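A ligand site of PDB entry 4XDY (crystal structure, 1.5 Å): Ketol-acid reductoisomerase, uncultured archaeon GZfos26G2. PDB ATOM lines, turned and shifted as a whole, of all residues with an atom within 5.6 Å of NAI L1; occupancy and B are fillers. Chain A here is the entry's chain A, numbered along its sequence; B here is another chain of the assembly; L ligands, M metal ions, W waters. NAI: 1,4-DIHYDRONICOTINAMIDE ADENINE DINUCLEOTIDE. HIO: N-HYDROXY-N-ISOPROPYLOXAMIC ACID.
The side-chain carboxylate (OD1) of Asp 87 is in hydrogen-bond range of an oxygen (O3D) of NAI L1 (2.6 Å). OE2 of Glu 46 is in hydrogen-bond range of O2B of NAI L1. OG of Ser 57 is in hydrogen-bond range of O3B of NAI L1 (2.8 Å). The backbone NH (N) of Gln 27 sits at hydrogen-bond distance from an oxygen (O2N) of NAI L1 (3.0 Å). The side-chain amide oxygen (OE1) of Gln 27 sits at hydrogen-bond distance from a nitrogen (N7N) of NAI L1. The side-chain amide nitrogen of Asn 55 lies within hydrogen-bond range of an oxygen (O2B) of NAI L1, at 3.0 Å. The backbone NH (N) of Ala 26 sits at hydrogen-bond distance from an oxygen (O2A) of NAI L1. O7N of NAI L1 sits at hydrogen-bond distance from N of Ser 256 of chain B (3.3 Å). NE2 of Gln 90 is in hydrogen-bond range of O3D of NAI L1. N of Ser 256 of chain B is in hydrogen-bond range of O12 of HIO L2. OG of Ser 256 of chain B sits close to O12 of HIO L2, at 3.5 Å.
OG1 of Thr 258 of chain B is in hydrogen-bond range of OD2 of Asp 87 (2.7 Å). The side-chain carboxylate of Glu 46 sits at hydrogen-bond distance from the side-chain amide nitrogen of Asn 55 (2.9 Å). The backbone NH (N) of Tyr 24 lies within hydrogen-bond range of the side-chain carboxylate (OE2) of Glu 46. OD1 of Asn 55 sits at hydrogen-bond distance from N of Ser 57 (3.1 Å). The backbone carbonyl oxygen (O) of Ala 136 sits close to the side-chain amide oxygen (OE1) of Gln 27 (3.0 Å). The backbone carbonyl oxygen (O) of Thr 47 sits at hydrogen-bond distance from the side-chain amide nitrogen (ND2) of Asn 55 (2.9 Å). N of Thr 258 of chain B lies close to OG of Ser 256 of chain B (3.4 Å). The backbone carbonyl oxygen (O) of Leu 85 is in hydrogen-bond range of the side-chain amide nitrogen (NE2) of Gln 90 (2.9 Å).
N7N of NAI L1 sits close to N of Gly 138 (3.0 Å). The backbone carbonyl oxygen of Val 254 of chain B sits close to an oxygen (O7N) of NAI L1 (2.9 Å). Gly 23 touches NAI L1. C of Tyr 24 touches O3B of NAI L1, at 3.9 Å. Gly 25 touches NAI L1. Leu 50 touches NAI L1 (CD1 to C4A, 3.6 Å). Leu 84 touches NAI L1. Leu 85 touches NAI L1. CD of Pro 86 touches O5B of NAI L1 (3.2 Å). Val 89 touches NAI L1 (CG1 to N6A, 3.6 Å). Ile 93 touches NAI L1 (CD1 to C2A, 3.4 Å). Ser 111 touches NAI L1 (O to C6N, 3.5 Å). CB of His 112 touches O2D of NAI L1, 3.4 Å away. Pro 134 touches NAI L1. Ala 136 touches NAI L1 (O to C4N, 3.4 Å). Pro 137 touches NAI L1 (CA to N7N, 3.3 Å). C of Ile 255 of chain B touches O7N of NAI L1, 3.5 Å away. Hydrophobic or aromatic side chains that line NAI L1: Ala 26, Leu 50, Leu 84, Leu 85, Pro 86, Val 89, Ile 93 and His 112. Along chain A the residues within 4 Å of NAI L1 span positions 23 to 138. The nearest printed residue that does not touch NAI L1 is Thr 47 (4.1 Å).
Water W12 bridges an oxygen (O1A) of NAI L1 (2.7 Å) and the backbone NH (N) of Asn 257 of chain B (3.0 Å). Water W10 lies within hydrogen-bond range of O3D of NAI L1, O of Ile 83, N of Ser 111 and NE2 of Gln 90. Water W1 lies within hydrogen-bond range of the backbone carbonyl oxygen (O) of Leu 84 (2.7 Å), an oxygen (O2N) of NAI L1 (2.8 Å), the backbone NH (N) of Gly 28 (2.8 Å), the backbone NH (N) of Gly 25 (2.9 Å) and the backbone carbonyl oxygen (O) of Gly 23 (3.4 Å). Water W3 lies within hydrogen-bond range of OG1 of Thr 47 (2.7 Å), OE1 of Glu 46 (2.7 Å) and N3A of NAI L1 (2.8 Å). Water W8 bridges O2D of NAI L1 and ND1 of His 112. Water W13 bridges O2A of NAI L1 (3.3 Å) and N of Ala 26 (3.4 Å).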
ATOM      1  N   GLY A  23     -15.733  20.707   8.161  1.00  0.00           N
ATOM      2  CA  GLY A  23     -14.831  21.829   8.479  1.00  0.00           C
ATOM      3  C   GLY A  23     -13.979  21.623   9.660  1.00  0.00           C
ATOM      4  O   GLY A  23     -14.485  21.572  10.777  1.00  0.00           O
ATOM      5  N   TYR A  24     -12.660  21.575   9.493  1.00  0.00           N
ATOM      6  CA  TYR A  24     -11.772  21.413  10.578  1.00  0.00           C
ATOM      7  C   TYR A  24     -11.038  22.700  10.888  1.00  0.00           C
ATOM      8  O   TYR A  24      -9.818  22.691  10.863  1.00  0.00           O
ATOM      9  CB  TYR A  24     -10.735  20.278  10.251  1.00  0.00           C
ATOM     10  CG  TYR A  24      -9.936  19.672  11.353  1.00  0.00           C
ATOM     11  CD1 TYR A  24     -10.479  18.731  12.211  1.00  0.00           C
ATOM     12  CD2 TYR A  24      -8.591  19.946  11.500  1.00  0.00           C
ATOM     13  CE1 TYR A  24      -9.762  18.136  13.217  1.00  0.00           C
ATOM     14  CE2 TYR A  24      -7.823  19.354  12.514  1.00  0.00           C
ATOM     15  CZ  TYR A  24      -8.412  18.394  13.362  1.00  0.00           C
ATOM     16  OH  TYR A  24      -7.733  17.801  14.385  1.00  0.00           O
ATOM     17  N   GLY A  25     -11.763  23.766  11.283  1.00  0.00           N
ATOM     18  CA  GLY A  25     -11.195  25.054  11.636  1.00  0.00           C
ATOM     19  C   GLY A  25     -11.337  25.277  13.122  1.00  0.00           C
ATOM     20  O   GLY A  25     -11.154  24.350  13.907  1.00  0.00           O
ATOM     21  N   ALA A  26     -11.587  26.506  13.560  1.00  0.00           N
ATOM     22  CA  ALA A  26     -11.457  26.791  15.031  1.00  0.00           C
ATOM     23  C   ALA A  26     -12.394  25.848  15.799  1.00  0.00           C
ATOM     24  O   ALA A  26     -11.983  25.220  16.795  1.00  0.00           O
ATOM     25  CB  ALA A  26     -11.873  28.241  15.301  1.00  0.00           C
ATOM     26  N   GLN A  27     -13.642  25.769  15.363  1.00  0.00           N
ATOM     27  CA  GLN A  27     -14.625  24.927  16.036  1.00  0.00           C
ATOM     28  C   GLN A  27     -14.506  23.419  15.661  1.00  0.00           C
ATOM     29  O   GLN A  27     -14.594  22.582  16.543  1.00  0.00           O
ATOM     30  CB  GLN A  27     -16.038  25.434  15.807  1.00  0.00           C
ATOM     31  CG  GLN A  27     -16.395  26.676  16.648  1.00  0.00           C
ATOM     32  CD  GLN A  27     -16.290  26.492  18.148  1.00  0.00           C
ATOM     33  OE1 GLN A  27     -15.948  27.436  18.904  1.00  0.00           O
ATOM     34  NE2 GLN A  27     -16.590  25.329  18.606  1.00  0.00           N
ATOM     35  N   GLY A  28     -14.348  23.095  14.399  1.00  0.00           N
ATOM     36  CA  GLY A  28     -14.298  21.710  13.960  1.00  0.00           C
ATOM     37  C   GLY A  28     -13.115  20.983  14.600  1.00  0.00           C
ATOM     38  O   GLY A  28     -13.241  19.833  15.050  1.00  0.00           O
ATOM     39  N   GLU A  46     -13.905  17.384   4.735  1.00  0.00           N
ATOM     40  CA  GLU A  46     -13.125  18.559   4.368  1.00  0.00           C
ATOM     41  C   GLU A  46     -12.903  18.585   2.890  1.00  0.00           C
ATOM     42  O   GLU A  46     -13.422  17.705   2.176  1.00  0.00           O
ATOM     43  CB  GLU A  46     -11.800  18.625   5.142  1.00  0.00           C
ATOM     44  CG  GLU A  46     -11.804  19.632   6.286  1.00  0.00           C
ATOM     45  CD  GLU A  46     -11.824  21.118   5.884  1.00  0.00           C
ATOM     46  OE1 GLU A  46     -11.932  21.430   4.700  1.00  0.00           O
ATOM     47  OE2 GLU A  46     -11.864  22.010   6.827  1.00  0.00           O
ATOM     48  N   THR A  47     -12.271  19.665   2.424  1.00  0.00           N
ATOM     49  CA  THR A  47     -11.984  19.878   1.035  1.00  0.00           C
ATOM     50  C   THR A  47     -10.452  19.973   0.856  1.00  0.00           C
ATOM     51  O   THR A  47      -9.783  20.790   1.493  1.00  0.00           O
ATOM     52  CB  THR A  47     -12.650  21.152   0.530  1.00  0.00           C
ATOM     53  OG1 THR A  47     -14.063  21.107   0.838  1.00  0.00           O
ATOM     54  CG2 THR A  47     -12.470  21.271  -0.999  1.00  0.00           C
ATOM     55  N   LEU A  50      -8.311  24.191  -1.658  1.00  0.00           N
ATOM     56  CA  LEU A  50      -9.101  25.399  -1.616  1.00  0.00           C
ATOM     57  C   LEU A  50      -8.312  26.548  -2.272  1.00  0.00           C
ATOM     58  O   LEU A  50      -7.127  26.677  -1.983  1.00  0.00           O
ATOM     59  CB  LEU A  50      -9.410  25.726  -0.133  1.00  0.00           C
ATOM     60  CG  LEU A  50     -10.675  25.092   0.463  1.00  0.00           C
ATOM     61  CD1 LEU A  50     -10.823  25.700   1.869  1.00  0.00           C
ATOM     62  CD2 LEU A  50     -11.943  25.325  -0.352  1.00  0.00           C
ATOM     63  N   ASN A  55      -5.412  22.607   1.046  1.00  0.00           N
ATOM     64  CA  ASN A  55      -6.040  23.142   2.251  1.00  0.00           C
ATOM     65  C   ASN A  55      -5.334  22.630   3.488  1.00  0.00           C
ATOM     66  O   ASN A  55      -5.359  21.455   3.756  1.00  0.00           O
ATOM     67  CB  ASN A  55      -7.520  22.735   2.244  1.00  0.00           C
ATOM     68  CG  ASN A  55      -8.267  23.236   3.473  1.00  0.00           C
ATOM     69  OD1 ASN A  55      -7.725  24.030   4.244  1.00  0.00           O
ATOM     70  ND2 ASN A  55      -9.518  22.768   3.663  1.00  0.00           N
ATOM     71  N   SER A  57      -6.218  22.621   6.534  1.00  0.00           N
ATOM     72  CA  SER A  57      -7.147  21.997   7.461  1.00  0.00           C
ATOM     73  C   SER A  57      -7.335  20.495   7.120  1.00  0.00           C
ATOM     74  O   SER A  57      -7.384  19.637   8.033  1.00  0.00           O
ATOM     75  CB  SER A  57      -8.496  22.714   7.352  1.00  0.00           C
ATOM     76  OG  SER A  57      -8.323  24.047   7.766  1.00  0.00           O
ATOM     77  N   TRP A  58      -7.430  20.193   5.836  1.00  0.00           N
ATOM     78  CA  TRP A  58      -7.405  18.795   5.378  1.00  0.00           C
ATOM     79  C   TRP A  58      -6.160  18.019   5.909  1.00  0.00           C
ATOM     80  O   TRP A  58      -6.262  16.957   6.528  1.00  0.00           O
ATOM     81  CB  TRP A  58      -7.525  18.780   3.837  1.00  0.00           C
ATOM     82  CG  TRP A  58      -7.420  17.393   3.227  1.00  0.00           C
ATOM     83  CD1 TRP A  58      -6.289  16.685   3.021  1.00  0.00           C
ATOM     84  CD2 TRP A  58      -8.508  16.570   2.729  1.00  0.00           C
ATOM     85  NE1 TRP A  58      -6.590  15.456   2.447  1.00  0.00           N
ATOM     86  CE2 TRP A  58      -7.936  15.377   2.224  1.00  0.00           C
ATOM     87  CE3 TRP A  58      -9.892  16.749   2.636  1.00  0.00           C
ATOM     88  CZ2 TRP A  58      -8.717  14.340   1.668  1.00  0.00           C
ATOM     89  CZ3 TRP A  58     -10.666  15.721   2.061  1.00  0.00           C
ATOM     90  CH2 TRP A  58     -10.077  14.531   1.595  1.00  0.00           C
ATOM     91  N   ILE A  71     -16.539  16.137   1.728  1.00  0.00           N
ATOM     92  CA  ILE A  71     -17.770  16.422   2.466  1.00  0.00           C
ATOM     93  C   ILE A  71     -18.919  15.481   2.072  1.00  0.00           C
ATOM     94  O   ILE A  71     -19.649  14.978   2.973  1.00  0.00           O
ATOM     95  CB  ILE A  71     -18.187  17.925   2.345  1.00  0.00           C
ATOM     96  CG1 ILE A  71     -17.100  18.787   3.027  1.00  0.00           C
ATOM     97  CG2 ILE A  71     -19.591  18.179   2.859  1.00  0.00           C
ATOM     98  CD1 ILE A  71     -17.241  20.279   2.832  1.00  0.00           C
ATOM     99  N   ILE A  83     -22.205  20.793  10.927  1.00  0.00           N
ATOM    100  CA  ILE A  83     -21.707  21.804   9.975  1.00  0.00           C
ATOM    101  C   ILE A  83     -20.887  22.823  10.755  1.00  0.00           C
ATOM    102  O   ILE A  83     -21.464  23.646  11.467  1.00  0.00           O
ATOM    103  CB  ILE A  83     -22.831  22.388   9.141  1.00  0.00           C
ATOM    104  CG1 ILE A  83     -23.429  21.280   8.232  1.00  0.00           C
ATOM    105  CG2 ILE A  83     -22.301  23.491   8.207  1.00  0.00           C
ATOM    106  CD1 ILE A  83     -24.646  21.678   7.491  1.00  0.00           C
ATOM    107  N   LEU A  84     -19.564  22.715  10.629  1.00  0.00           N
ATOM    108  CA  LEU A  84     -18.622  23.666  11.267  1.00  0.00           C
ATOM    109  C   LEU A  84     -17.742  24.367  10.201  1.00  0.00           C
ATOM    110  O   LEU A  84     -16.599  24.649  10.436  1.00  0.00           O
ATOM    111  CB  LEU A  84     -17.849  23.010  12.385  1.00  0.00           C
ATOM    112  CG  LEU A  84     -18.632  22.521  13.594  1.00  0.00           C
ATOM    113  CD1 LEU A  84     -17.782  21.782  14.613  1.00  0.00           C
ATOM    114  CD2 LEU A  84     -19.405  23.664  14.245  1.00  0.00           C
ATOM    115  N   LEU A  85     -18.400  24.671   9.090  1.00  0.00           N
ATOM    116  CA  LEU A  85     -17.863  25.487   8.058  1.00  0.00           C
ATOM    117  C   LEU A  85     -18.210  26.972   8.350  1.00  0.00           C
ATOM    118  O   LEU A  85     -19.158  27.264   9.040  1.00  0.00           O
ATOM    119  CB  LEU A  85     -18.465  25.061   6.728  1.00  0.00           C
ATOM    120  CG  LEU A  85     -18.078  23.667   6.250  1.00  0.00           C
ATOM    121  CD1 LEU A  85     -19.064  23.154   5.220  1.00  0.00           C
ATOM    122  CD2 LEU A  85     -16.689  23.633   5.680  1.00  0.00           C
ATOM    123  N   PRO A  86     -17.494  27.920   7.709  1.00  0.00           N
ATOM    124  CA  PRO A  86     -17.898  29.343   7.868  1.00  0.00           C
ATOM    125  C   PRO A  86     -19.337  29.555   7.526  1.00  0.00           C
ATOM    126  O   PRO A  86     -19.855  29.004   6.548  1.00  0.00           O
ATOM    127  CB  PRO A  86     -16.944  30.090   6.882  1.00  0.00           C
ATOM    128  CG  PRO A  86     -15.742  29.201   6.743  1.00  0.00           C
ATOM    129  CD  PRO A  86     -16.360  27.767   6.803  1.00  0.00           C
ATOM    130  N   ASP A  87     -20.056  30.353   8.310  1.00  0.00           N
ATOM    131  CA  ASP A  87     -21.494  30.573   8.075  1.00  0.00           C
ATOM    132  C   ASP A  87     -21.800  30.963   6.640  1.00  0.00           C
ATOM    133  O   ASP A  87     -22.786  30.513   6.054  1.00  0.00           O
ATOM    134  CB  ASP A  87     -22.127  31.597   9.014  1.00  0.00           C
ATOM    135  CG  ASP A  87     -21.935  31.211  10.476  1.00  0.00           C
ATOM    136  OD1 ASP A  87     -22.576  30.185  10.895  1.00  0.00           O
ATOM    137  OD2 ASP A  87     -21.098  31.843  11.168  1.00  0.00           O
ATOM    138  N   VAL A  89     -20.443  30.330   3.797  1.00  0.00           N
ATOM    139  CA  VAL A  89     -20.314  29.312   2.747  1.00  0.00           C
ATOM    140  C   VAL A  89     -21.229  28.095   2.968  1.00  0.00           C
ATOM    141  O   VAL A  89     -21.439  27.302   2.050  1.00  0.00           O
ATOM    142  CB  VAL A  89     -18.900  28.796   2.510  1.00  0.00           C
ATOM    143  CG1 VAL A  89     -18.006  29.984   2.014  1.00  0.00           C
ATOM    144  CG2 VAL A  89     -18.283  28.119   3.690  1.00  0.00           C
ATOM    145  N   GLN A  90     -21.836  28.001   4.163  1.00  0.00           N
ATOM    146  CA  GLN A  90     -22.684  26.801   4.416  1.00  0.00           C
ATOM    147  C   GLN A  90     -23.778  26.628   3.408  1.00  0.00           C
ATOM    148  O   GLN A  90     -24.022  25.466   3.020  1.00  0.00           O
ATOM    149  CB  GLN A  90     -23.243  26.837   5.798  1.00  0.00           C
ATOM    150  CG  GLN A  90     -22.215  26.778   6.898  1.00  0.00           C
ATOM    151  CD  GLN A  90     -22.854  26.780   8.287  1.00  0.00           C
ATOM    152  OE1 GLN A  90     -24.080  26.758   8.441  1.00  0.00           O
ATOM    153  NE2 GLN A  90     -21.990  26.919   9.329  1.00  0.00           N
ATOM    154  N   ILE A  93     -22.479  24.857   0.101  1.00  0.00           N
ATOM    155  CA  ILE A  93     -21.894  23.603   0.362  1.00  0.00           C
ATOM    156  C   ILE A  93     -22.996  22.607   0.812  1.00  0.00           C
ATOM    157  O   ILE A  93     -23.046  21.451   0.384  1.00  0.00           O
ATOM    158  CB  ILE A  93     -20.757  23.714   1.394  1.00  0.00           C
ATOM    159  CG1 ILE A  93     -19.588  24.487   0.737  1.00  0.00           C
ATOM    160  CG2 ILE A  93     -20.281  22.337   1.735  1.00  0.00           C
ATOM    161  CD1 ILE A  93     -18.471  24.772   1.665  1.00  0.00           C
ATOM    162  N   SER A 111     -23.337  24.866  15.036  1.00  0.00           N
ATOM    163  CA  SER A 111     -22.930  25.506  16.273  1.00  0.00           C
ATOM    164  C   SER A 111     -23.240  26.983  16.325  1.00  0.00           C
ATOM    165  O   SER A 111     -22.813  27.649  17.249  1.00  0.00           O
ATOM    166  CB  SER A 111     -21.490  25.258  16.625  1.00  0.00           C
ATOM    167  OG  SER A 111     -21.266  23.910  17.052  1.00  0.00           O
ATOM    168  N   HIS A 112     -24.071  27.447  15.394  1.00  0.00           N
ATOM    169  CA  HIS A 112     -24.604  28.804  15.413  1.00  0.00           C
ATOM    170  C   HIS A 112     -25.886  28.697  14.614  1.00  0.00           C
ATOM    171  O   HIS A 112     -25.880  28.054  13.513  1.00  0.00           O
ATOM    172  CB  HIS A 112     -23.635  29.741  14.700  1.00  0.00           C
ATOM    173  CG  HIS A 112     -24.043  31.177  14.666  1.00  0.00           C
ATOM    174  ND1 HIS A 112     -24.756  31.828  15.691  1.00  0.00           N
ATOM    175  CD2 HIS A 112     -23.819  32.114  13.709  1.00  0.00           C
ATOM    176  CE1 HIS A 112     -24.871  33.118  15.361  1.00  0.00           C
ATOM    177  NE2 HIS A 112     -24.305  33.308  14.168  1.00  0.00           N
ATOM    178  N   PRO A 134     -21.278  26.551  21.409  1.00  0.00           N
ATOM    179  CA  PRO A 134     -20.446  26.850  22.554  1.00  0.00           C
ATOM    180  C   PRO A 134     -20.317  28.365  22.656  1.00  0.00           C
ATOM    181  O   PRO A 134     -20.092  28.994  21.636  1.00  0.00           O
ATOM    182  CB  PRO A 134     -19.082  26.182  22.203  1.00  0.00           C
ATOM    183  CG  PRO A 134     -19.068  26.195  20.710  1.00  0.00           C
ATOM    184  CD  PRO A 134     -20.471  26.220  20.218  1.00  0.00           C
ATOM    185  N   ALA A 136     -17.823  30.244  23.333  1.00  0.00           N
ATOM    186  CA  ALA A 136     -16.401  30.188  23.454  1.00  0.00           C
ATOM    187  C   ALA A 136     -15.728  30.134  22.086  1.00  0.00           C
ATOM    188  O   ALA A 136     -16.213  29.457  21.172  1.00  0.00           O
ATOM    189  CB  ALA A 136     -15.958  28.985  24.215  1.00  0.00           C
ATOM    190  N   PRO A 137     -14.595  30.848  21.960  1.00  0.00           N
ATOM    191  CA  PRO A 137     -13.742  30.575  20.823  1.00  0.00           C
ATOM    192  C   PRO A 137     -13.140  29.126  20.866  1.00  0.00           C
ATOM    193  O   PRO A 137     -12.800  28.600  21.924  1.00  0.00           O
ATOM    194  CB  PRO A 137     -12.645  31.641  20.912  1.00  0.00           C
ATOM    195  CG  PRO A 137     -12.574  31.935  22.369  1.00  0.00           C
ATOM    196  CD  PRO A 137     -13.960  31.743  22.916  1.00  0.00           C
ATOM    197  N   GLY A 138     -12.939  28.545  19.704  1.00  0.00           N
ATOM    198  CA  GLY A 138     -12.659  27.126  19.662  1.00  0.00           C
ATOM    199  C   GLY A 138     -11.349  26.708  20.340  1.00  0.00           C
ATOM    200  O   GLY A 138     -11.281  25.644  20.953  1.00  0.00           O
ATOM    201  N   ASP A 195     -26.047  35.756  20.199  1.00  0.00           N
ATOM    202  CA  ASP A 195     -24.639  35.481  19.770  1.00  0.00           C
ATOM    203  C   ASP A 195     -24.116  36.632  18.912  1.00  0.00           C
ATOM    204  O   ASP A 195     -23.032  37.131  19.157  1.00  0.00           O
ATOM    205  CB  ASP A 195     -24.582  34.179  18.988  1.00  0.00           C
ATOM    206  CG  ASP A 195     -23.147  33.780  18.688  1.00  0.00           C
ATOM    207  OD1 ASP A 195     -22.474  33.297  19.619  1.00  0.00           O
ATOM    208  OD2 ASP A 195     -22.721  34.062  17.543  1.00  0.00           O
ATOM    209  N   VAL B 254      -9.332  33.461  15.084  1.00  0.00           N
ATOM    210  CA  VAL B 254      -9.975  32.309  15.761  1.00  0.00           C
ATOM    211  C   VAL B 254     -11.491  32.456  15.745  1.00  0.00           C
ATOM    212  O   VAL B 254     -12.205  31.493  15.533  1.00  0.00           O
ATOM    213  CB  VAL B 254      -9.466  32.171  17.220  1.00  0.00           C
ATOM    214  CG1 VAL B 254     -10.266  31.141  17.958  1.00  0.00           C
ATOM    215  CG2 VAL B 254      -7.981  31.813  17.227  1.00  0.00           C
ATOM    216  N   ILE B 255     -11.979  33.669  15.901  1.00  0.00           N
ATOM    217  CA  ILE B 255     -13.437  33.897  15.891  1.00  0.00           C
ATOM    218  C   ILE B 255     -13.937  33.660  14.456  1.00  0.00           C
ATOM    219  O   ILE B 255     -13.137  33.622  13.495  1.00  0.00           O
ATOM    220  CB  ILE B 255     -13.841  35.318  16.329  1.00  0.00           C
ATOM    221  CG1 ILE B 255     -13.426  36.378  15.270  1.00  0.00           C
ATOM    222  CG2 ILE B 255     -13.377  35.596  17.722  1.00  0.00           C
ATOM    223  CD1 ILE B 255     -13.779  37.784  15.679  1.00  0.00           C
ATOM    224  N   SER B 256     -15.224  33.490  14.323  1.00  0.00           N
ATOM    225  CA  SER B 256     -15.768  33.266  12.991  1.00  0.00           C
ATOM    226  C   SER B 256     -15.616  34.444  12.102  1.00  0.00           C
ATOM    227  O   SER B 256     -15.549  35.572  12.570  1.00  0.00           O
ATOM    228  CB  SER B 256     -17.224  32.850  13.051  1.00  0.00           C
ATOM    229  OG  SER B 256     -18.082  33.906  13.413  1.00  0.00           O
ATOM    230  N   ASN B 257     -15.693  34.203  10.776  1.00  0.00           N
ATOM    231  CA  ASN B 257     -15.760  35.335   9.847  1.00  0.00           C
ATOM    232  C   ASN B 257     -16.995  36.192  10.103  1.00  0.00           C
ATOM    233  O   ASN B 257     -16.942  37.445   9.995  1.00  0.00           O
ATOM    234  CB  ASN B 257     -15.649  34.905   8.405  1.00  0.00           C
ATOM    235  CG  ASN B 257     -14.391  34.126   8.156  1.00  0.00           C
ATOM    236  OD1 ASN B 257     -13.327  34.319   8.788  1.00  0.00           O
ATOM    237  ND2 ASN B 257     -14.526  33.148   7.265  1.00  0.00           N
ATOM    238  N   THR B 258     -18.117  35.569  10.503  1.00  0.00           N
ATOM    239  CA  THR B 258     -19.297  36.293  10.854  1.00  0.00           C
ATOM    240  C   THR B 258     -19.030  37.314  11.970  1.00  0.00           C
ATOM    241  O   THR B 258     -19.438  38.478  11.863  1.00  0.00           O
ATOM    242  CB  THR B 258     -20.426  35.319  11.298  1.00  0.00           C
ATOM    243  OG1 THR B 258     -20.649  34.385  10.234  1.00  0.00           O
ATOM    244  CG2 THR B 258     -21.702  36.017  11.638  1.00  0.00           C
HETATM  245  PA  NAI L   1     -13.673  28.319  10.001  1.00  0.00           P
HETATM  246  O1A NAI L   1     -13.735  29.720   9.384  1.00  0.00           O
HETATM  247  O2A NAI L   1     -12.604  27.979  10.942  1.00  0.00           O
HETATM  248  O5B NAI L   1     -13.875  27.297   8.764  1.00  0.00           O
HETATM  249  C5B NAI L   1     -13.760  25.863   8.981  1.00  0.00           C
HETATM  250  C4B NAI L   1     -12.980  25.257   7.768  1.00  0.00           C
HETATM  251  O4B NAI L   1     -13.848  25.414   6.652  1.00  0.00           O
HETATM  252  C3B NAI L   1     -11.645  25.920   7.341  1.00  0.00           C
HETATM  253  O3B NAI L   1     -10.632  25.494   8.258  1.00  0.00           O
HETATM  254  C2B NAI L   1     -11.506  25.437   5.906  1.00  0.00           C
HETATM  255  O2B NAI L   1     -10.813  24.187   5.917  1.00  0.00           O
HETATM  256  C1B NAI L   1     -12.989  25.263   5.495  1.00  0.00           C
HETATM  257  N9A NAI L   1     -13.379  26.250   4.510  1.00  0.00           N
HETATM  258  C8A NAI L   1     -13.094  27.615   4.633  1.00  0.00           C
HETATM  259  N7A NAI L   1     -13.582  28.256   3.577  1.00  0.00           N
HETATM  260  C5A NAI L   1     -14.132  27.312   2.766  1.00  0.00           C
HETATM  261  C6A NAI L   1     -14.774  27.329   1.468  1.00  0.00           C
HETATM  262  N6A NAI L   1     -14.940  28.459   0.776  1.00  0.00           N
HETATM  263  N1A NAI L   1     -15.269  26.171   0.942  1.00  0.00           N
HETATM  264  C2A NAI L   1     -15.102  25.001   1.590  1.00  0.00           C
HETATM  265  N3A NAI L   1     -14.524  24.882   2.776  1.00  0.00           N
HETATM  266  C4A NAI L   1     -14.015  26.003   3.399  1.00  0.00           C
HETATM  267  O3  NAI L   1     -15.168  28.088  10.769  1.00  0.00           O
HETATM  268  PN  NAI L   1     -15.411  28.445  12.383  1.00  0.00           P
HETATM  269  O1N NAI L   1     -14.990  29.869  12.666  1.00  0.00           O
HETATM  270  O2N NAI L   1     -14.795  27.344  13.130  1.00  0.00           O
HETATM  271  O5D NAI L   1     -16.995  28.485  12.303  1.00  0.00           O
HETATM  272  C5D NAI L   1     -17.725  27.218  12.237  1.00  0.00           C
HETATM  273  C4D NAI L   1     -19.184  27.390  12.782  1.00  0.00           C
HETATM  274  O4D NAI L   1     -18.995  27.556  14.204  1.00  0.00           O
HETATM  275  C3D NAI L   1     -19.930  28.633  12.338  1.00  0.00           C
HETATM  276  O3D NAI L   1     -21.339  28.357  12.235  1.00  0.00           O
HETATM  277  C2D NAI L   1     -19.691  29.684  13.441  1.00  0.00           C
HETATM  278  O2D NAI L   1     -20.646  30.743  13.536  1.00  0.00           O
HETATM  279  C1D NAI L   1     -19.675  28.787  14.661  1.00  0.00           C
HETATM  280  N1N NAI L   1     -18.968  29.229  15.866  1.00  0.00           N
HETATM  281  C2N NAI L   1     -17.664  29.570  15.763  1.00  0.00           C
HETATM  282  C3N NAI L   1     -16.960  29.957  16.849  1.00  0.00           C
HETATM  283  C7N NAI L   1     -15.562  30.204  16.727  1.00  0.00           C
HETATM  284  O7N NAI L   1     -14.921  30.498  15.672  1.00  0.00           O
HETATM  285  N7N NAI L   1     -14.881  29.860  17.792  1.00  0.00           N
HETATM  286  C4N NAI L   1     -17.639  29.988  18.137  1.00  0.00           C
HETATM  287  C5N NAI L   1     -18.942  29.411  18.195  1.00  0.00           C
HETATM  288  C6N NAI L   1     -19.572  29.077  17.042  1.00  0.00           C
HETATM  289  C1  HIO L   2     -18.073  33.586  16.778  1.00  0.00           C
HETATM  290  O11 HIO L   2     -18.968  33.772  15.904  1.00  0.00           O
HETATM  291  O12 HIO L   2     -16.829  33.350  16.612  1.00  0.00           O
HETATM  292  C2  HIO L   2     -18.693  33.569  18.175  1.00  0.00           C
HETATM  293  O2  HIO L   2     -19.942  33.418  18.256  1.00  0.00           O
HETATM  294  N3  HIO L   2     -18.008  33.830  19.279  1.00  0.00           N
HETATM  295  O3  HIO L   2     -18.573  33.456  20.570  1.00  0.00           O
HETATM  296  C4  HIO L   2     -16.696  34.402  19.279  1.00  0.00           C
HETATM  297  C41 HIO L   2     -16.684  35.581  20.263  1.00  0.00           C
HETATM  298  C42 HIO L   2     -15.746  33.277  19.656  1.00  0.00           C
HETATM  299 MG    MG M   1     -11.566  33.589   9.662  1.00  0.00          MG
HETATM  300 MG    MG M   2     -20.884  33.986  16.616  1.00  0.00          MG
HETATM  301 MG    MG M   3     -20.544  33.417  20.186  1.00  0.00          MG
HETATM  302  O   HOH W   1     -14.426  24.738  12.075  1.00  0.00           O
HETATM  303  O   HOH W   2     -12.394  30.665  12.766  1.00  0.00           O
HETATM  304  O   HOH W   3     -14.171  22.113   3.328  1.00  0.00           O
HETATM  305  O   HOH W   4     -16.457  28.766  -1.559  1.00  0.00           O
HETATM  306  O   HOH W   5     -20.796  31.238  20.124  1.00  0.00           O
HETATM  307  O   HOH W   6     -12.364  31.924  10.182  1.00  0.00           O
HETATM  308  O   HOH W   7     -15.767  25.060  -1.405  1.00  0.00           O
HETATM  309  O   HOH W   8     -21.311  31.943  16.079  1.00  0.00           O
HETATM  310  O   HOH W   9     -10.273  28.132   9.648  1.00  0.00           O
HETATM  311  O   HOH W  10     -22.586  25.938  12.567  1.00  0.00           O
HETATM  312  O   HOH W  11     -22.574  30.378  18.035  1.00  0.00           O
HETATM  313  O   HOH W  12     -15.750  31.242  10.236  1.00  0.00           O
HETATM  314  O   HOH W  13     -10.072  29.362  12.474  1.00  0.00           O
